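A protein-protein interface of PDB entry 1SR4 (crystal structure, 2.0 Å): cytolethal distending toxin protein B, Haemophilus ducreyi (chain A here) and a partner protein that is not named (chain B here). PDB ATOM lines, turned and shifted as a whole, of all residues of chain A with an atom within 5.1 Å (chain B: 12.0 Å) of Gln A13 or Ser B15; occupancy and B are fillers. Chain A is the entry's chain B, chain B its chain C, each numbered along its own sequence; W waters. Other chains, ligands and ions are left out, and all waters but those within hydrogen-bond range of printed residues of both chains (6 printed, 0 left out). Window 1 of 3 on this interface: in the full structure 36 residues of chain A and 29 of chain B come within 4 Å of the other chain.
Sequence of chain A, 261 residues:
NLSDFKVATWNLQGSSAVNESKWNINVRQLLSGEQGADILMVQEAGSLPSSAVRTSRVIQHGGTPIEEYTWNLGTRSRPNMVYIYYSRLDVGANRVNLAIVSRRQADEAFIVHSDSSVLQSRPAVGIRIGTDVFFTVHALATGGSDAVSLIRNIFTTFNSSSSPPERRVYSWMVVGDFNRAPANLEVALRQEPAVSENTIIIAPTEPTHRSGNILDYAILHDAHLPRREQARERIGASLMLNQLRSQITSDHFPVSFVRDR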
ATOM      1  N   ASN A  11      15.172  12.981 -35.488  1.00  0.00           N
ATOM      2  CA  ASN A  11      14.848  14.323 -35.044  1.00  0.00           C
ATOM      3  C   ASN A  11      15.194  14.232 -33.560  1.00  0.00           C
ATOM      4  O   ASN A  11      14.526  13.540 -32.794  1.00  0.00           O
ATOM      5  CB  ASN A  11      13.354  14.650 -35.219  1.00  0.00           C
ATOM      6  CG  ASN A  11      13.030  16.067 -34.781  1.00  0.00           C
ATOM      7  OD1 ASN A  11      13.674  16.607 -33.873  1.00  0.00           O
ATOM      8  ND2 ASN A  11      12.038  16.671 -35.402  1.00  0.00           N
ATOM      9  N   LEU A  12      16.259  14.917 -33.181  1.00  0.00           N
ATOM     10  CA  LEU A  12      16.773  14.918 -31.823  1.00  0.00           C
ATOM     11  C   LEU A  12      15.949  15.712 -30.807  1.00  0.00           C
ATOM     12  O   LEU A  12      16.049  15.458 -29.606  1.00  0.00           O
ATOM     13  CB  LEU A  12      18.227  15.432 -31.872  1.00  0.00           C
ATOM     14  CG  LEU A  12      19.159  15.414 -30.649  1.00  0.00           C
ATOM     15  CD1 LEU A  12      20.587  15.061 -31.108  1.00  0.00           C
ATOM     16  CD2 LEU A  12      19.141  16.802 -29.939  1.00  0.00           C
ATOM     17  N   GLN A  13      15.137  16.658 -31.281  1.00  0.00           N
ATOM     18  CA  GLN A  13      14.313  17.506 -30.402  1.00  0.00           C
ATOM     19  C   GLN A  13      15.166  18.109 -29.296  1.00  0.00           C
ATOM     20  O   GLN A  13      14.842  18.006 -28.112  1.00  0.00           O
ATOM     21  CB  GLN A  13      13.150  16.707 -29.781  1.00  0.00           C
ATOM     22  CG  GLN A  13      12.127  16.209 -30.820  1.00  0.00           C
ATOM     23  CD  GLN A  13      10.840  15.708 -30.194  1.00  0.00           C
ATOM     24  OE1 GLN A  13      10.856  14.912 -29.258  1.00  0.00           O
ATOM     25  NE2 GLN A  13       9.712  16.172 -30.712  1.00  0.00           N
ATOM     26  N   GLY A  14      16.240  18.776 -29.684  1.00  0.00           N
ATOM     27  CA  GLY A  14      17.124  19.357 -28.689  1.00  0.00           C
ATOM     28  C   GLY A  14      16.608  20.638 -28.057  1.00  0.00           C
ATOM     29  O   GLY A  14      15.716  21.292 -28.604  1.00  0.00           O
ATOM     30  N   SER A  15      17.157  20.991 -26.897  1.00  0.00           N
ATOM     31  CA  SER A  15      16.787  22.225 -26.212  1.00  0.00           C
ATOM     32  C   SER A  15      17.881  22.599 -25.227  1.00  0.00           C
ATOM     33  O   SER A  15      18.832  21.845 -25.011  1.00  0.00           O
ATOM     34  CB  SER A  15      15.469  22.072 -25.449  1.00  0.00           C
ATOM     35  OG  SER A  15      15.608  21.121 -24.412  1.00  0.00           O
ATOM     36  N   VAL A  18      18.025  19.877 -22.448  1.00  0.00           N
ATOM     37  CA  VAL A  18      18.565  18.550 -22.776  1.00  0.00           C
ATOM     38  C   VAL A  18      19.009  18.551 -24.239  1.00  0.00           C
ATOM     39  O   VAL A  18      18.197  18.798 -25.138  1.00  0.00           O
ATOM     40  CB  VAL A  18      17.497  17.451 -22.576  1.00  0.00           C
ATOM     41  CG1 VAL A  18      18.174  16.070 -22.517  1.00  0.00           C
ATOM     42  CG2 VAL A  18      16.702  17.717 -21.292  1.00  0.00           C
ATOM     43  N   LYS A  22      21.732  13.672 -25.515  1.00  0.00           N
ATOM     44  CA  LYS A  22      21.113  13.000 -26.662  1.00  0.00           C
ATOM     45  C   LYS A  22      22.133  12.637 -27.745  1.00  0.00           C
ATOM     46  O   LYS A  22      22.050  11.569 -28.357  1.00  0.00           O
ATOM     47  CB  LYS A  22      19.998  13.869 -27.262  1.00  0.00           C
ATOM     48  CG  LYS A  22      18.932  14.320 -26.239  1.00  0.00           C
ATOM     49  CD  LYS A  22      17.651  14.796 -26.938  1.00  0.00           C
ATOM     50  CE  LYS A  22      16.631  15.351 -25.948  1.00  0.00           C
ATOM     51  NZ  LYS A  22      15.281  15.478 -26.615  1.00  0.00           N
ATOM     52  N   GLN A  43      17.597  16.616 -37.126  1.00  0.00           N
ATOM     53  CA  GLN A  43      16.758  17.811 -37.115  1.00  0.00           C
ATOM     54  C   GLN A  43      16.692  18.240 -35.653  1.00  0.00           C
ATOM     55  O   GLN A  43      16.929  17.430 -34.767  1.00  0.00           O
ATOM     56  CB  GLN A  43      15.363  17.516 -37.660  1.00  0.00           C
ATOM     57  CG  GLN A  43      15.328  16.962 -39.078  1.00  0.00           C
ATOM     58  CD  GLN A  43      15.593  15.468 -39.120  1.00  0.00           C
ATOM     59  OE1 GLN A  43      14.999  14.709 -38.362  1.00  0.00           O
ATOM     60  NE2 GLN A  43      16.485  15.037 -40.011  1.00  0.00           N
ATOM     61  N   GLU A  44      16.396  19.508 -35.399  1.00  0.00           N
ATOM     62  CA  GLU A  44      16.329  20.027 -34.034  1.00  0.00           C
ATOM     63  C   GLU A  44      17.604  19.618 -33.296  1.00  0.00           C
ATOM     64  O   GLU A  44      17.581  19.142 -32.153  1.00  0.00           O
ATOM     65  CB  GLU A  44      15.076  19.492 -33.330  1.00  0.00           C
ATOM     66  CG  GLU A  44      13.771  19.978 -33.990  1.00  0.00           C
ATOM     67  CD  GLU A  44      12.542  19.631 -33.188  1.00  0.00           C
ATOM     68  OE1 GLU A  44      12.549  19.890 -31.958  1.00  0.00           O
ATOM     69  OE2 GLU A  44      11.575  19.108 -33.787  1.00  0.00           O
ATOM     70  N   HIS A 209       7.072   8.369 -34.718  1.00  0.00           N
ATOM     71  CA  HIS A 209       6.861   9.396 -33.685  1.00  0.00           C
ATOM     72  C   HIS A 209       5.881   8.823 -32.670  1.00  0.00           C
ATOM     73  O   HIS A 209       5.056   7.978 -33.011  1.00  0.00           O
ATOM     74  CB  HIS A 209       6.305  10.663 -34.335  1.00  0.00           C
ATOM     75  CG  HIS A 209       6.073  11.792 -33.379  1.00  0.00           C
ATOM     76  ND1 HIS A 209       4.812  12.254 -33.071  1.00  0.00           N
ATOM     77  CD2 HIS A 209       6.940  12.580 -32.698  1.00  0.00           C
ATOM     78  CE1 HIS A 209       4.909  13.274 -32.237  1.00  0.00           C
ATOM     79  NE2 HIS A 209       6.191  13.492 -31.992  1.00  0.00           N
ATOM     80  N   SER A 250      14.063  11.224 -27.570  1.00  0.00           N
ATOM     81  CA  SER A 250      13.177  12.203 -28.201  1.00  0.00           C
ATOM     82  C   SER A 250      11.893  11.445 -28.561  1.00  0.00           C
ATOM     83  O   SER A 250      11.829  10.214 -28.440  1.00  0.00           O
ATOM     84  CB  SER A 250      13.807  12.814 -29.454  1.00  0.00           C
ATOM     85  OG  SER A 250      13.532  12.021 -30.577  1.00  0.00           O
ATOM     86  N   ASP A 251      10.862  12.159 -28.981  1.00  0.00           N
ATOM     87  CA  ASP A 251       9.616  11.485 -29.337  1.00  0.00           C
ATOM     88  C   ASP A 251       9.646  10.879 -30.750  1.00  0.00           C
ATOM     89  O   ASP A 251       8.651  10.326 -31.198  1.00  0.00           O
ATOM     90  CB  ASP A 251       8.427  12.448 -29.211  1.00  0.00           C
ATOM     91  CG  ASP A 251       8.082  12.767 -27.765  1.00  0.00           C
ATOM     92  OD1 ASP A 251       8.459  11.988 -26.863  1.00  0.00           O
ATOM     93  OD2 ASP A 251       7.413  13.795 -27.538  1.00  0.00           O
ATOM     94  N   HIS A 252      10.780  11.002 -31.450  1.00  0.00           N
ATOM     95  CA  HIS A 252      10.927  10.448 -32.792  1.00  0.00           C
ATOM     96  C   HIS A 252      11.853   9.239 -32.740  1.00  0.00           C
ATOM     97  O   HIS A 252      12.812   9.196 -31.955  1.00  0.00           O
ATOM     98  CB  HIS A 252      11.537  11.472 -33.752  1.00  0.00           C
ATOM     99  CG  HIS A 252      10.623  12.607 -34.102  1.00  0.00           C
ATOM    100  ND1 HIS A 252       9.888  12.637 -35.268  1.00  0.00           N
ATOM    101  CD2 HIS A 252      10.320  13.746 -33.434  1.00  0.00           C
ATOM    102  CE1 HIS A 252       9.172  13.749 -35.306  1.00  0.00           C
ATOM    103  NE2 HIS A 252       9.416  14.439 -34.204  1.00  0.00           N
ATOM    104  N   ASP B   5      11.192  29.135 -25.325  1.00  0.00           N
ATOM    105  CA  ASP B   5      12.001  30.371 -25.546  1.00  0.00           C
ATOM    106  C   ASP B   5      11.675  31.044 -26.878  1.00  0.00           C
ATOM    107  O   ASP B   5      10.815  30.571 -27.626  1.00  0.00           O
ATOM    108  CB  ASP B   5      13.494  30.041 -25.462  1.00  0.00           C
ATOM    109  CG  ASP B   5      14.049  30.216 -24.056  1.00  0.00           C
ATOM    110  OD1 ASP B   5      13.283  30.671 -23.167  1.00  0.00           O
ATOM    111  OD2 ASP B   5      15.250  29.907 -23.853  1.00  0.00           O
ATOM    112  N   PRO B   6      12.368  32.149 -27.201  1.00  0.00           N
ATOM    113  CA  PRO B   6      12.095  32.849 -28.454  1.00  0.00           C
ATOM    114  C   PRO B   6      12.739  32.214 -29.676  1.00  0.00           C
ATOM    115  O   PRO B   6      13.561  32.840 -30.343  1.00  0.00           O
ATOM    116  CB  PRO B   6      12.641  34.242 -28.174  1.00  0.00           C
ATOM    117  CG  PRO B   6      13.892  33.924 -27.448  1.00  0.00           C
ATOM    118  CD  PRO B   6      13.453  32.828 -26.466  1.00  0.00           C
ATOM    119  N   THR B   7      12.356  30.980 -29.984  1.00  0.00           N
ATOM    120  CA  THR B   7      12.927  30.311 -31.140  1.00  0.00           C
ATOM    121  C   THR B   7      12.535  31.008 -32.438  1.00  0.00           C
ATOM    122  O   THR B   7      11.458  31.593 -32.547  1.00  0.00           O
ATOM    123  CB  THR B   7      12.475  28.828 -31.229  1.00  0.00           C
ATOM    124  OG1 THR B   7      12.959  28.261 -32.449  1.00  0.00           O
ATOM    125  CG2 THR B   7      10.962  28.722 -31.215  1.00  0.00           C
ATOM    126  N   TYR B   9      11.817  29.531 -34.994  1.00  0.00           N
ATOM    127  CA  TYR B   9      10.806  28.693 -35.636  1.00  0.00           C
ATOM    128  C   TYR B   9       9.709  28.264 -34.685  1.00  0.00           C
ATOM    129  O   TYR B   9       9.691  27.125 -34.204  1.00  0.00           O
ATOM    130  CB  TYR B   9      11.486  27.465 -36.241  1.00  0.00           C
ATOM    131  CG  TYR B   9      12.510  27.835 -37.290  1.00  0.00           C
ATOM    132  CD1 TYR B   9      12.114  28.253 -38.565  1.00  0.00           C
ATOM    133  CD2 TYR B   9      13.870  27.818 -36.992  1.00  0.00           C
ATOM    134  CE1 TYR B   9      13.050  28.641 -39.513  1.00  0.00           C
ATOM    135  CE2 TYR B   9      14.811  28.210 -37.924  1.00  0.00           C
ATOM    136  CZ  TYR B   9      14.401  28.622 -39.180  1.00  0.00           C
ATOM    137  OH  TYR B   9      15.351  29.034 -40.089  1.00  0.00           O
ATOM    138  N   PRO B  10       8.751  29.162 -34.423  1.00  0.00           N
ATOM    139  CA  PRO B  10       7.649  28.858 -33.506  1.00  0.00           C
ATOM    140  C   PRO B  10       6.700  27.718 -33.876  1.00  0.00           C
ATOM    141  O   PRO B  10       5.842  27.363 -33.071  1.00  0.00           O
ATOM    142  CB  PRO B  10       6.936  30.204 -33.369  1.00  0.00           C
ATOM    143  CG  PRO B  10       7.182  30.850 -34.703  1.00  0.00           C
ATOM    144  CD  PRO B  10       8.638  30.536 -34.941  1.00  0.00           C
ATOM    145  N   ASP B  11       6.821  27.152 -35.072  1.00  0.00           N
ATOM    146  CA  ASP B  11       5.952  26.034 -35.413  1.00  0.00           C
ATOM    147  C   ASP B  11       6.461  24.795 -34.683  1.00  0.00           C
ATOM    148  O   ASP B  11       5.754  23.799 -34.571  1.00  0.00           O
ATOM    149  CB  ASP B  11       5.919  25.769 -36.935  1.00  0.00           C
ATOM    150  CG  ASP B  11       7.256  25.267 -37.489  1.00  0.00           C
ATOM    151  OD1 ASP B  11       8.262  25.982 -37.343  1.00  0.00           O
ATOM    152  OD2 ASP B  11       7.294  24.159 -38.074  1.00  0.00           O
ATOM    153  N   VAL B  12       7.682  24.868 -34.166  1.00  0.00           N
ATOM    154  CA  VAL B  12       8.281  23.730 -33.470  1.00  0.00           C
ATOM    155  C   VAL B  12       8.150  23.855 -31.962  1.00  0.00           C
ATOM    156  O   VAL B  12       8.784  24.712 -31.338  1.00  0.00           O
ATOM    157  CB  VAL B  12       9.792  23.584 -33.796  1.00  0.00           C
ATOM    158  CG1 VAL B  12      10.355  22.353 -33.092  1.00  0.00           C
ATOM    159  CG2 VAL B  12      10.005  23.474 -35.304  1.00  0.00           C
ATOM    160  N   GLU B  13       7.335  22.997 -31.367  1.00  0.00           N
ATOM    161  CA  GLU B  13       7.172  23.044 -29.924  1.00  0.00           C
ATOM    162  C   GLU B  13       8.442  22.639 -29.174  1.00  0.00           C
ATOM    163  O   GLU B  13       9.299  21.934 -29.701  1.00  0.00           O
ATOM    164  CB  GLU B  13       6.026  22.131 -29.481  1.00  0.00           C
ATOM    165  CG  GLU B  13       4.636  22.761 -29.593  1.00  0.00           C
ATOM    166  CD  GLU B  13       3.693  22.259 -28.508  1.00  0.00           C
ATOM    167  OE1 GLU B  13       3.316  23.053 -27.601  1.00  0.00           O
ATOM    168  OE2 GLU B  13       3.346  21.064 -28.565  1.00  0.00           O
ATOM    169  N   LEU B  14       8.548  23.106 -27.938  1.00  0.00           N
ATOM    170  CA  LEU B  14       9.669  22.784 -27.061  1.00  0.00           C
ATOM    171  C   LEU B  14       9.321  21.428 -26.428  1.00  0.00           C
ATOM    172  O   LEU B  14       8.210  21.260 -25.909  1.00  0.00           O
ATOM    173  CB  LEU B  14       9.779  23.843 -25.963  1.00  0.00           C
ATOM    174  CG  LEU B  14      10.851  23.684 -24.876  1.00  0.00           C
ATOM    175  CD1 LEU B  14      12.242  23.886 -25.492  1.00  0.00           C
ATOM    176  CD2 LEU B  14      10.630  24.713 -23.774  1.00  0.00           C
ATOM    177  N   SER B  15      10.250  20.475 -26.482  1.00  0.00           N
ATOM    178  CA  SER B  15      10.038  19.142 -25.907  1.00  0.00           C
ATOM    179  C   SER B  15      10.607  19.053 -24.496  1.00  0.00           C
ATOM    180  O   SER B  15      11.713  19.526 -24.235  1.00  0.00           O
ATOM    181  CB  SER B  15      10.740  18.059 -26.741  1.00  0.00           C
ATOM    182  OG  SER B  15      10.109  17.858 -27.987  1.00  0.00           O
ATOM    183  N   PRO B  16       9.868  18.427 -23.567  1.00  0.00           N
ATOM    184  CA  PRO B  16      10.366  18.299 -22.188  1.00  0.00           C
ATOM    185  C   PRO B  16      11.474  17.232 -22.101  1.00  0.00           C
ATOM    186  O   PRO B  16      11.750  16.530 -23.070  1.00  0.00           O
ATOM    187  CB  PRO B  16       9.107  17.910 -21.406  1.00  0.00           C
ATOM    188  CG  PRO B  16       8.350  17.083 -22.403  1.00  0.00           C
ATOM    189  CD  PRO B  16       8.506  17.872 -23.698  1.00  0.00           C
ATOM    190  N   PRO B  17      12.123  17.100 -20.938  1.00  0.00           N
ATOM    191  CA  PRO B  17      13.193  16.102 -20.790  1.00  0.00           C
ATOM    192  C   PRO B  17      12.710  14.654 -20.992  1.00  0.00           C
ATOM    193  O   PRO B  17      11.569  14.314 -20.671  1.00  0.00           O
ATOM    194  CB  PRO B  17      13.690  16.343 -19.367  1.00  0.00           C
ATOM    195  CG  PRO B  17      13.407  17.824 -19.150  1.00  0.00           C
ATOM    196  CD  PRO B  17      12.006  17.922 -19.722  1.00  0.00           C
ATOM    197  N   PRO B  18      13.580  13.786 -21.530  1.00  0.00           N
ATOM    198  CA  PRO B  18      13.216  12.388 -21.756  1.00  0.00           C
ATOM    199  C   PRO B  18      13.066  11.622 -20.439  1.00  0.00           C
ATOM    200  O   PRO B  18      13.759  11.907 -19.455  1.00  0.00           O
ATOM    201  CB  PRO B  18      14.376  11.859 -22.601  1.00  0.00           C
ATOM    202  CG  PRO B  18      15.525  12.665 -22.139  1.00  0.00           C
ATOM    203  CD  PRO B  18      14.960  14.052 -21.977  1.00  0.00           C
ATOM    204  N   ARG B  19      12.158  10.652 -20.439  1.00  0.00           N
ATOM    205  CA  ARG B  19      11.889   9.819 -19.278  1.00  0.00           C
ATOM    206  C   ARG B  19      12.715   8.531 -19.407  1.00  0.00           C
ATOM    207  O   ARG B  19      12.787   7.959 -20.486  1.00  0.00           O
ATOM    208  CB  ARG B  19      10.404   9.460 -19.239  1.00  0.00           C
ATOM    209  CG  ARG B  19       9.954   8.798 -17.955  1.00  0.00           C
ATOM    210  CD  ARG B  19       9.834   9.836 -16.851  1.00  0.00           C
ATOM    211  NE  ARG B  19       8.780  10.804 -17.151  1.00  0.00           N
ATOM    212  CZ  ARG B  19       7.488  10.597 -16.919  1.00  0.00           C
ATOM    213  NH1 ARG B  19       7.074   9.449 -16.380  1.00  0.00           N
ATOM    214  NH2 ARG B  19       6.604  11.545 -17.216  1.00  0.00           N
ATOM    215  N   GLU B  47      13.753  11.839 -14.922  1.00  0.00           N
ATOM    216  CA  GLU B  47      13.803  12.706 -16.086  1.00  0.00           C
ATOM    217  C   GLU B  47      15.287  12.999 -16.234  1.00  0.00           C
ATOM    218  O   GLU B  47      15.964  13.350 -15.257  1.00  0.00           O
ATOM    219  CB  GLU B  47      13.035  14.004 -15.836  1.00  0.00           C
ATOM    220  CG  GLU B  47      11.549  13.756 -15.592  1.00  0.00           C
ATOM    221  CD  GLU B  47      10.798  15.017 -15.218  1.00  0.00           C
ATOM    222  OE1 GLU B  47      11.443  15.976 -14.735  1.00  0.00           O
ATOM    223  OE2 GLU B  47       9.560  15.035 -15.391  1.00  0.00           O
ATOM    224  N   LEU B  48      15.800  12.848 -17.449  1.00  0.00           N
ATOM    225  CA  LEU B  48      17.209  13.080 -17.677  1.00  0.00           C
ATOM    226  C   LEU B  48      17.407  14.519 -18.110  1.00  0.00           C
ATOM    227  O   LEU B  48      16.926  14.905 -19.157  1.00  0.00           O
ATOM    228  CB  LEU B  48      17.727  12.121 -18.759  1.00  0.00           C
ATOM    229  CG  LEU B  48      19.235  12.171 -19.043  1.00  0.00           C
ATOM    230  CD1 LEU B  48      19.991  11.617 -17.829  1.00  0.00           C
ATOM    231  CD2 LEU B  48      19.572  11.335 -20.296  1.00  0.00           C
ATOM    232  N   ILE B  49      18.108  15.319 -17.310  1.00  0.00           N
ATOM    233  CA  ILE B  49      18.330  16.710 -17.688  1.00  0.00           C
ATOM    234  C   ILE B  49      19.823  17.031 -17.708  1.00  0.00           C
ATOM    235  O   ILE B  49      20.580  16.549 -16.871  1.00  0.00           O
ATOM    236  CB  ILE B  49      17.581  17.678 -16.729  1.00  0.00           C
ATOM    237  CG1 ILE B  49      18.122  17.550 -15.312  1.00  0.00           C
ATOM    238  CG2 ILE B  49      16.083  17.360 -16.712  1.00  0.00           C
ATOM    239  CD1 ILE B  49      19.275  18.488 -15.037  1.00  0.00           C
ATOM    240  N   ASP B  50      20.255  17.835 -18.672  1.00  0.00           N
ATOM    241  CA  ASP B  50      21.672  18.171 -18.769  1.00  0.00           C
ATOM    242  C   ASP B  50      22.043  19.316 -17.846  1.00  0.00           C
ATOM    243  O   ASP B  50      21.323  20.303 -17.769  1.00  0.00           O
ATOM    244  CB  ASP B  50      22.043  18.557 -20.204  1.00  0.00           C
ATOM    245  CG  ASP B  50      21.894  17.400 -21.173  1.00  0.00           C
ATOM    246  OD1 ASP B  50      21.597  16.279 -20.713  1.00  0.00           O
ATOM    247  OD2 ASP B  50      22.076  17.607 -22.387  1.00  0.00           O
ATOM    248  N   LYS B  52      24.081  22.530 -16.969  1.00  0.00           N
ATOM    249  CA  LYS B  52      24.732  23.578 -17.742  1.00  0.00           C
ATOM    250  C   LYS B  52      25.814  24.388 -17.033  1.00  0.00           C
ATOM    251  O   LYS B  52      26.485  25.202 -17.670  1.00  0.00           O
ATOM    252  CB  LYS B  52      23.671  24.538 -18.288  1.00  0.00           C
ATOM    253  CG  LYS B  52      22.458  23.846 -18.912  1.00  0.00           C
ATOM    254  CD  LYS B  52      22.855  22.865 -20.013  1.00  0.00           C
ATOM    255  CE  LYS B  52      23.460  23.566 -21.223  1.00  0.00           C
ATOM    256  NZ  LYS B  52      22.470  24.399 -21.953  1.00  0.00           N
ATOM    257  N   LYS B  69      16.296  13.616 -12.383  1.00  0.00           N
ATOM    258  CA  LYS B  69      15.210  14.283 -11.669  1.00  0.00           C
ATOM    259  C   LYS B  69      13.939  13.465 -11.498  1.00  0.00           C
ATOM    260  O   LYS B  69      13.513  12.738 -12.396  1.00  0.00           O
ATOM    261  CB  LYS B  69      14.877  15.596 -12.391  1.00  0.00           C
ATOM    262  CG  LYS B  69      13.751  16.420 -11.773  1.00  0.00           C
ATOM    263  CD  LYS B  69      13.388  17.589 -12.690  1.00  0.00           C
ATOM    264  CE  LYS B  69      12.104  18.297 -12.236  1.00  0.00           C
ATOM    265  NZ  LYS B  69      10.963  17.339 -12.128  1.00  0.00           N
ATOM    266  N   LEU B 156       2.382   1.615 -30.312  1.00  0.00           N
ATOM    267  CA  LEU B 156       2.032   2.722 -31.196  1.00  0.00           C
ATOM    268  C   LEU B 156       1.320   2.194 -32.441  1.00  0.00           C
ATOM    269  O   LEU B 156       1.762   1.223 -33.054  1.00  0.00           O
ATOM    270  CB  LEU B 156       3.295   3.500 -31.607  1.00  0.00           C
ATOM    271  CG  LEU B 156       4.046   4.182 -30.462  1.00  0.00           C
ATOM    272  CD1 LEU B 156       5.340   4.795 -30.979  1.00  0.00           C
ATOM    273  CD2 LEU B 156       3.160   5.229 -29.823  1.00  0.00           C
HETATM  274  O   HOH W   1      14.479  18.995 -25.559  1.00  0.00           O
HETATM  275  O   HOH W   2      10.829  19.836 -29.995  1.00  0.00           O
HETATM  276  O   HOH W   3      14.198  16.605 -24.400  1.00  0.00           O
HETATM  277  O   HOH W   4      21.780  22.248 -23.753  1.00  0.00           O
HETATM  278  O   HOH W   5      13.423  20.464 -22.481  1.00  0.00           O
HETATM  279  O   HOH W   6      12.656  20.787 -27.744  1.00  0.00           O
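Water W2 lies within hydrogen-bond range of OE1 of Glu A44 (2.6 Å), O of Glu B13 (2.6 Å) and OG of Ser B15 (2.9 Å). Water W5 bridges the backbone carbonyl oxygen of Ser B15 (2.6 Å) and the side-chain hydroxyl of Ser A15 (3.0 Å). Water W1 lies within hydrogen-bond range of OG of Ser A15 (2.7 Å), O of Gln A13 (2.8 Å) and O of Ser B15 (3.1 Å). Water W3 lies within hydrogen-bond range of NZ of Lys A22 and O of Pro B16. Water W6 lies within hydrogen-bond range of the backbone NH (N) of Ser B15 (2.7 Å) and the backbone carbonyl oxygen (O) of Gly A14 (3.2 Å). Water W4 lies within hydrogen-bond range of the side-chain amino group (NZ) of Lys B52 (2.9 Å) and the backbone carbonyl oxygen (O) of Ser A15 (3.2 Å).
OD1 of Asn A11 is in hydrogen-bond range of N of Gln A13, 3.0 Å away. The side-chain carboxylate (OE2) of Glu A44 lies within hydrogen-bond range of the side-chain amide nitrogen (ND2) of Asn A11 (3.0 Å). The backbone carbonyl oxygen of Gln A13 sits at hydrogen-bond distance from the side-chain amino group of Lys A22, at 3.0 Å. The side-chain amide oxygen of Gln A13 is in hydrogen-bond range of the backbone NH of Asp A251. OG of Ser A15 sits at hydrogen-bond distance from N of Val A18 (3.4 Å). The backbone NH of Leu B48 lies within hydrogen-bond range of the backbone carbonyl oxygen of Pro B18 (3.0 Å).
Of chain B, only Ser B15 (3.2 Å) comes within 4 Å of Gln A13. Ser B15 touches just one residue of chain A: Gln A13. No residue of chain B comes within 4 Å of Asn A11. No residue of chain B comes within 4 Å of Leu A12. No residue of chain B comes within 4 Å of Gly A14. No residue of chain B comes within 4 Å of Ser A250. No residue of chain B comes within 4 Å of Asp A251. Printed residues of chain A within 4 Å of Pro B18: Val A18 (3.8 Å). Of the printed residues of chain A, Leu B156 touches His A209 (3.8 Å). Printed residues of chain A within 4 Å of Pro B17: Val A18 (3.8 Å). Printed residues of chain A within 4 Å of Leu B14: Ser A15 (3.7 Å). Lys B69 touches none of the printed residues of chain A. Pro B6 touches none of the printed residues of chain A. The nearest residue of chain B that does not touch Gln A13 is Glu B13 (5.9 Å). The nearest residue of chain A that does not touch Ser B15 is Ser A15 (4.2 Å).
Hydrophobic or aromatic side chains of chain A that line the printed part of chain B: Val A18. Among the printed residues, 8 pairs touch across the chains.
Leu B14 touches Ser A15 (CD1 to CB, 3.7 Å). CG2 of Val A18 touches CB of Pro B17, 3.8 Å away. Val A18 touches Pro B18. Val A18 touches Leu B48 (CG2 to O, 3.5 Å). Asp B50 touches Val A18. Glu A44 touches Val B12 (OE1 to CG1, 3.5 Å). His A209 touches Leu B156 (O to CD1, 3.8 Å).
OG of Ser B15 sits close to NE2 of Gln A13 (3.2 Å).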
